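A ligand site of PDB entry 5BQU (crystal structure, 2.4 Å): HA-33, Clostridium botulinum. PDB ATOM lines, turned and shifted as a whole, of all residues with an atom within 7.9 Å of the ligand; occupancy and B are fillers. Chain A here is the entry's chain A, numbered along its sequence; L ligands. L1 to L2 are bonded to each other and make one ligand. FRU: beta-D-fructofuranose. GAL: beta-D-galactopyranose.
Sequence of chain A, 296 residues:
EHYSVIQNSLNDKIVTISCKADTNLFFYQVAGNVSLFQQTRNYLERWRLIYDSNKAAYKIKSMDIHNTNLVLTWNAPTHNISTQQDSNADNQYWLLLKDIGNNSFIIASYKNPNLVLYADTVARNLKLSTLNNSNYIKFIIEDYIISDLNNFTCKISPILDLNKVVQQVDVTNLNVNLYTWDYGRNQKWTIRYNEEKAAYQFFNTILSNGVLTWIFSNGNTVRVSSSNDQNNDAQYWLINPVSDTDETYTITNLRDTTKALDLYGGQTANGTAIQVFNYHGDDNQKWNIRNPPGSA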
ATOM      1  N   ASN A 220     -19.573  20.127  -9.840  1.00  0.00           N
ATOM      2  CA  ASN A 220     -19.368  20.813 -11.140  1.00  0.00           C
ATOM      3  C   ASN A 220     -18.007  21.523 -11.321  1.00  0.00           C
ATOM      4  O   ASN A 220     -17.740  22.072 -12.383  1.00  0.00           O
ATOM      5  CB  ASN A 220     -20.476  21.860 -11.386  1.00  0.00           C
ATOM      6  CG  ASN A 220     -21.819  21.230 -11.708  1.00  0.00           C
ATOM      7  OD1 ASN A 220     -21.894  20.090 -12.141  1.00  0.00           O
ATOM      8  ND2 ASN A 220     -22.878  21.987 -11.505  1.00  0.00           N
ATOM      9  N   ALA A 260     -21.431  19.693 -20.100  1.00  0.00           N
ATOM     10  CA  ALA A 260     -20.763  20.602 -21.047  1.00  0.00           C
ATOM     11  C   ALA A 260     -19.966  21.654 -20.293  1.00  0.00           C
ATOM     12  O   ALA A 260     -20.416  22.162 -19.273  1.00  0.00           O
ATOM     13  CB  ALA A 260     -21.798  21.263 -21.940  1.00  0.00           C
ATOM     14  N   LEU A 261     -18.780  21.987 -20.801  1.00  0.00           N
ATOM     15  CA  LEU A 261     -17.994  23.052 -20.201  1.00  0.00           C
ATOM     16  C   LEU A 261     -18.845  24.312 -20.248  1.00  0.00           C
ATOM     17  O   LEU A 261     -19.469  24.595 -21.271  1.00  0.00           O
ATOM     18  CB  LEU A 261     -16.681  23.246 -20.970  1.00  0.00           C
ATOM     19  CG  LEU A 261     -15.621  24.133 -20.308  1.00  0.00           C
ATOM     20  CD1 LEU A 261     -14.959  23.423 -19.135  1.00  0.00           C
ATOM     21  CD2 LEU A 261     -14.587  24.541 -21.352  1.00  0.00           C
ATOM     22  N   ASP A 262     -18.900  25.035 -19.135  1.00  0.00           N
ATOM     23  CA  ASP A 262     -19.877  26.118 -18.954  1.00  0.00           C
ATOM     24  C   ASP A 262     -19.327  27.321 -18.166  1.00  0.00           C
ATOM     25  O   ASP A 262     -18.591  27.155 -17.194  1.00  0.00           O
ATOM     26  CB  ASP A 262     -21.142  25.578 -18.262  1.00  0.00           C
ATOM     27  CG  ASP A 262     -22.305  26.546 -18.320  1.00  0.00           C
ATOM     28  OD1 ASP A 262     -22.060  27.743 -18.594  1.00  0.00           O
ATOM     29  OD2 ASP A 262     -23.479  26.132 -18.132  1.00  0.00           O
ATOM     30  N   LEU A 263     -19.721  28.507 -18.619  1.00  0.00           N
ATOM     31  CA  LEU A 263     -19.390  29.778 -17.951  1.00  0.00           C
ATOM     32  C   LEU A 263     -20.496  30.092 -16.941  1.00  0.00           C
ATOM     33  O   LEU A 263     -21.669  30.186 -17.310  1.00  0.00           O
ATOM     34  CB  LEU A 263     -19.256  30.922 -18.977  1.00  0.00           C
ATOM     35  CG  LEU A 263     -19.045  32.356 -18.495  1.00  0.00           C
ATOM     36  CD1 LEU A 263     -17.710  32.503 -17.801  1.00  0.00           C
ATOM     37  CD2 LEU A 263     -19.167  33.326 -19.665  1.00  0.00           C
ATOM     38  N   TYR A 264     -20.104  30.274 -15.676  1.00  0.00           N
ATOM     39  CA  TYR A 264     -21.060  30.485 -14.582  1.00  0.00           C
ATOM     40  C   TYR A 264     -21.999  31.651 -14.858  1.00  0.00           C
ATOM     41  O   TYR A 264     -21.569  32.793 -15.018  1.00  0.00           O
ATOM     42  CB  TYR A 264     -20.332  30.687 -13.249  1.00  0.00           C
ATOM     43  CG  TYR A 264     -21.234  30.477 -12.042  1.00  0.00           C
ATOM     44  CD1 TYR A 264     -21.270  29.242 -11.382  1.00  0.00           C
ATOM     45  CD2 TYR A 264     -22.037  31.506 -11.545  1.00  0.00           C
ATOM     46  CE1 TYR A 264     -22.091  29.042 -10.271  1.00  0.00           C
ATOM     47  CE2 TYR A 264     -22.856  31.307 -10.443  1.00  0.00           C
ATOM     48  CZ  TYR A 264     -22.879  30.076  -9.801  1.00  0.00           C
ATOM     49  OH  TYR A 264     -23.698  29.887  -8.709  1.00  0.00           O
ATOM     50  N   GLY A 265     -23.295  31.341 -14.932  1.00  0.00           N
ATOM     51  CA  GLY A 265     -24.373  32.319 -15.055  1.00  0.00           C
ATOM     52  C   GLY A 265     -24.341  33.181 -16.305  1.00  0.00           C
ATOM     53  O   GLY A 265     -24.976  34.252 -16.343  1.00  0.00           O
ATOM     54  N   GLY A 266     -23.621  32.722 -17.320  1.00  0.00           N
ATOM     55  CA  GLY A 266     -23.242  33.553 -18.452  1.00  0.00           C
ATOM     56  C   GLY A 266     -22.691  34.909 -18.021  1.00  0.00           C
ATOM     57  O   GLY A 266     -22.860  35.896 -18.740  1.00  0.00           O
ATOM     58  N   GLN A 267     -22.028  34.958 -16.865  1.00  0.00           N
ATOM     59  CA  GLN A 267     -21.433  36.198 -16.331  1.00  0.00           C
ATOM     60  C   GLN A 267     -20.097  36.416 -17.032  1.00  0.00           C
ATOM     61  O   GLN A 267     -19.369  35.466 -17.304  1.00  0.00           O
ATOM     62  CB  GLN A 267     -21.217  36.119 -14.812  1.00  0.00           C
ATOM     63  CG  GLN A 267     -22.456  35.857 -13.982  1.00  0.00           C
ATOM     64  CD  GLN A 267     -23.480  36.958 -14.085  1.00  0.00           C
ATOM     65  OE1 GLN A 267     -23.123  38.108 -14.351  1.00  0.00           O
ATOM     66  NE2 GLN A 267     -24.748  36.626 -13.880  1.00  0.00           N
ATOM     67  N   THR A 272     -15.009  35.145 -12.806  1.00  0.00           N
ATOM     68  CA  THR A 272     -16.134  34.243 -13.052  1.00  0.00           C
ATOM     69  C   THR A 272     -15.660  32.796 -13.256  1.00  0.00           C
ATOM     70  O   THR A 272     -14.752  32.544 -14.035  1.00  0.00           O
ATOM     71  CB  THR A 272     -16.928  34.670 -14.303  1.00  0.00           C
ATOM     72  OG1 THR A 272     -17.212  36.071 -14.258  1.00  0.00           O
ATOM     73  CG2 THR A 272     -18.235  33.898 -14.412  1.00  0.00           C
ATOM     74  N   ALA A 273     -16.299  31.859 -12.561  1.00  0.00           N
ATOM     75  CA  ALA A 273     -15.898  30.453 -12.613  1.00  0.00           C
ATOM     76  C   ALA A 273     -16.208  29.770 -13.960  1.00  0.00           C
ATOM     77  O   ALA A 273     -17.256  30.000 -14.560  1.00  0.00           O
ATOM     78  CB  ALA A 273     -16.553  29.684 -11.470  1.00  0.00           C
ATOM     79  N   GLN A 275     -16.943  26.105 -15.217  1.00  0.00           N
ATOM     80  CA  GLN A 275     -17.317  24.830 -14.647  1.00  0.00           C
ATOM     81  C   GLN A 275     -18.049  24.005 -15.688  1.00  0.00           C
ATOM     82  O   GLN A 275     -18.304  24.493 -16.787  1.00  0.00           O
ATOM     83  CB  GLN A 275     -18.206  25.031 -13.418  1.00  0.00           C
ATOM     84  CG  GLN A 275     -19.579  25.652 -13.665  1.00  0.00           C
ATOM     85  CD  GLN A 275     -20.425  25.769 -12.404  1.00  0.00           C
ATOM     86  OE1 GLN A 275     -21.640  25.877 -12.493  1.00  0.00           O
ATOM     87  NE2 GLN A 275     -19.795  25.750 -11.228  1.00  0.00           N
ATOM     88  N   VAL A 276     -18.341  22.745 -15.377  1.00  0.00           N
ATOM     89  CA  VAL A 276     -19.224  21.954 -16.231  1.00  0.00           C
ATOM     90  C   VAL A 276     -20.672  22.107 -15.761  1.00  0.00           C
ATOM     91  O   VAL A 276     -20.939  22.456 -14.603  1.00  0.00           O
ATOM     92  CB  VAL A 276     -18.842  20.452 -16.294  1.00  0.00           C
ATOM     93  CG1 VAL A 276     -17.543  20.275 -17.072  1.00  0.00           C
ATOM     94  CG2 VAL A 276     -18.746  19.839 -14.909  1.00  0.00           C
ATOM     95  N   PHE A 277     -21.596  21.861 -16.666  1.00  0.00           N
ATOM     96  CA  PHE A 277     -23.017  22.036 -16.393  1.00  0.00           C
ATOM     97  C   PHE A 277     -23.798  21.284 -17.470  1.00  0.00           C
ATOM     98  O   PHE A 277     -23.319  21.144 -18.602  1.00  0.00           O
ATOM     99  CB  PHE A 277     -23.391  23.522 -16.401  1.00  0.00           C
ATOM    100  CG  PHE A 277     -24.692  23.833 -15.696  1.00  0.00           C
ATOM    101  CD1 PHE A 277     -24.718  24.003 -14.320  1.00  0.00           C
ATOM    102  CD2 PHE A 277     -25.873  23.966 -16.411  1.00  0.00           C
ATOM    103  CE1 PHE A 277     -25.914  24.298 -13.656  1.00  0.00           C
ATOM    104  CE2 PHE A 277     -27.072  24.251 -15.769  1.00  0.00           C
ATOM    105  CZ  PHE A 277     -27.098  24.420 -14.393  1.00  0.00           C
ATOM    106  N   ASN A 278     -24.975  20.792 -17.095  1.00  0.00           N
ATOM    107  CA  ASN A 278     -25.832  20.029 -18.003  1.00  0.00           C
ATOM    108  C   ASN A 278     -26.022  20.753 -19.348  1.00  0.00           C
ATOM    109  O   ASN A 278     -26.338  21.945 -19.386  1.00  0.00           O
ATOM    110  CB  ASN A 278     -27.204  19.754 -17.365  1.00  0.00           C
ATOM    111  CG  ASN A 278     -27.554  18.285 -17.355  1.00  0.00           C
ATOM    112  OD1 ASN A 278     -26.775  17.457 -16.862  1.00  0.00           O
ATOM    113  ND2 ASN A 278     -28.723  17.955 -17.866  1.00  0.00           N
ATOM    114  N   HIS A 280     -27.423  22.446 -22.191  1.00  0.00           N
ATOM    115  CA  HIS A 280     -28.617  23.064 -22.782  1.00  0.00           C
ATOM    116  C   HIS A 280     -28.345  23.776 -24.128  1.00  0.00           C
ATOM    117  O   HIS A 280     -29.276  24.127 -24.859  1.00  0.00           O
ATOM    118  CB  HIS A 280     -29.368  23.998 -21.800  1.00  0.00           C
ATOM    119  CG  HIS A 280     -28.489  24.787 -20.875  1.00  0.00           C
ATOM    120  ND1 HIS A 280     -27.428  25.552 -21.316  1.00  0.00           N
ATOM    121  CD2 HIS A 280     -28.553  24.980 -19.535  1.00  0.00           C
ATOM    122  CE1 HIS A 280     -26.858  26.157 -20.280  1.00  0.00           C
ATOM    123  NE2 HIS A 280     -27.520  25.818 -19.189  1.00  0.00           N
ATOM    124  N   ASP A 282     -27.161  26.751 -24.692  1.00  0.00           N
ATOM    125  CA  ASP A 282     -27.319  28.200 -24.650  1.00  0.00           C
ATOM    126  C   ASP A 282     -25.979  28.837 -24.952  1.00  0.00           C
ATOM    127  O   ASP A 282     -24.966  28.138 -25.047  1.00  0.00           O
ATOM    128  CB  ASP A 282     -27.803  28.659 -23.272  1.00  0.00           C
ATOM    129  CG  ASP A 282     -29.213  28.222 -22.979  1.00  0.00           C
ATOM    130  OD1 ASP A 282     -29.930  27.890 -23.942  1.00  0.00           O
ATOM    131  OD2 ASP A 282     -29.594  28.228 -21.787  1.00  0.00           O
ATOM    132  N   ASN A 284     -23.895  30.581 -23.230  1.00  0.00           N
ATOM    133  CA  ASN A 284     -22.870  30.323 -22.197  1.00  0.00           C
ATOM    134  C   ASN A 284     -22.169  28.962 -22.279  1.00  0.00           C
ATOM    135  O   ASN A 284     -21.246  28.721 -21.521  1.00  0.00           O
ATOM    136  CB  ASN A 284     -23.449  30.504 -20.786  1.00  0.00           C
ATOM    137  CG  ASN A 284     -24.430  29.421 -20.404  1.00  0.00           C
ATOM    138  OD1 ASN A 284     -24.409  28.902 -19.303  1.00  0.00           O
ATOM    139  ND2 ASN A 284     -25.300  29.085 -21.326  1.00  0.00           N
ATOM    140  N   GLN A 285     -22.641  28.077 -23.161  1.00  0.00           N
ATOM    141  CA  GLN A 285     -21.983  26.783 -23.400  1.00  0.00           C
ATOM    142  C   GLN A 285     -21.320  26.731 -24.795  1.00  0.00           C
ATOM    143  O   GLN A 285     -20.881  25.693 -25.243  1.00  0.00           O
ATOM    144  CB  GLN A 285     -22.988  25.628 -23.222  1.00  0.00           C
ATOM    145  CG  GLN A 285     -23.515  25.483 -21.783  1.00  0.00           C
ATOM    146  CD  GLN A 285     -24.491  24.313 -21.580  1.00  0.00           C
ATOM    147  OE1 GLN A 285     -25.141  23.841 -22.519  1.00  0.00           O
ATOM    148  NE2 GLN A 285     -24.610  23.862 -20.328  1.00  0.00           N
HETATM  149  C1  FRU L   1     -29.724  34.230 -14.372  1.00  0.00           C
HETATM  150  C2  FRU L   1     -29.964  32.880 -13.719  1.00  0.00           C
HETATM  151  C3  FRU L   1     -28.649  32.213 -13.353  1.00  0.00           C
HETATM  152  C4  FRU L   1     -28.691  30.849 -13.960  1.00  0.00           C
HETATM  153  C5  FRU L   1     -29.895  30.830 -14.905  1.00  0.00           C
HETATM  154  C6  FRU L   1     -30.711  29.608 -14.520  1.00  0.00           C
HETATM  155  O1  FRU L   1     -30.920  34.675 -15.026  1.00  0.00           O
HETATM  156  O2  FRU L   1     -30.762  33.051 -12.546  1.00  0.00           O
HETATM  157  O3  FRU L   1     -28.533  32.104 -11.928  1.00  0.00           O
HETATM  158  O4  FRU L   1     -27.447  30.718 -14.623  1.00  0.00           O
HETATM  159  O5  FRU L   1     -30.640  32.023 -14.650  1.00  0.00           O
HETATM  160  O6  FRU L   1     -30.138  28.440 -15.125  1.00  0.00           O
HETATM  161  C1  GAL L   2     -26.967  29.387 -14.532  1.00  0.00           C
HETATM  162  C2  GAL L   2     -26.479  29.134 -15.935  1.00  0.00           C
HETATM  163  C3  GAL L   2     -25.807  27.767 -16.023  1.00  0.00           C
HETATM  164  C4  GAL L   2     -24.773  27.591 -14.921  1.00  0.00           C
HETATM  165  C5  GAL L   2     -25.347  27.960 -13.568  1.00  0.00           C
HETATM  166  C6  GAL L   2     -24.283  27.852 -12.476  1.00  0.00           C
HETATM  167  O2  GAL L   2     -27.581  29.187 -16.844  1.00  0.00           O
HETATM  168  O3  GAL L   2     -25.181  27.622 -17.299  1.00  0.00           O
HETATM  169  O4  GAL L   2     -23.633  28.410 -15.199  1.00  0.00           O
HETATM  170  O5  GAL L   2     -25.878  29.290 -13.618  1.00  0.00           O
HETATM  171  O6  GAL L   2     -24.363  26.568 -11.858  1.00  0.00           O
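CE1 of Tyr 264 touches C6 of GAL L2, at 3.3 Å.
CE1 of Phe 277 touches O6 of GAL L2 (3.3 Å).
NE2 of His 280 touches O3 of GAL L2, at 3.5 Å.
Hydrophobic or aromatic side chains that line the ligand: Tyr 264, Phe 277 and His 280.
The backbone NH (N) of His 280 is in hydrogen-bond range of the side-chain amide oxygen (OE1) of Gln 285 (2.7 Å).
The side-chain carboxylate (OD1) of Asp 262 lies close to the side-chain amide oxygen (OD1) of Asn 284 (2.7 Å).
The backbone carbonyl oxygen (O) of Phe 277 lies within hydrogen-bond range of the side-chain amide nitrogen (NE2) of Gln 285 (3.5 Å).
The backbone NH of Tyr 264 sits at hydrogen-bond distance from the backbone carbonyl oxygen of Ala 273, 3.1 Å away.
OD2 of Asp 282 is in hydrogen-bond range of ND1 of His 280, at 3.5 Å.
The side-chain amide nitrogen (NE2) of Gln 267 sits at hydrogen-bond distance from the backbone carbonyl oxygen (O) of Gly 265 (3.4 Å).
N of Leu 263 is in hydrogen-bond range of O of Asn 284, 3.3 Å away.
O of Phe 277 lies within hydrogen-bond range of N of Ala 260 (2.8 Å).
O6 of GAL L2 sits at hydrogen-bond distance from OE1 of Gln 275 (2.9 Å).
An oxygen (O4) of GAL L2 sits at hydrogen-bond distance from the backbone NH (N) of Gly 265 (3.0 Å).
OD1 of Asn 284 lies within hydrogen-bond range of O3 of GAL L2, 2.5 Å away.
An oxygen (O3) of GAL L2 is in hydrogen-bond range of the side-chain carboxylate (OD2) of Asp 262 (2.4 Å).
The backbone carbonyl oxygen of Leu 263 sits at hydrogen-bond distance from an oxygen (O4) of GAL L2 (3.4 Å).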
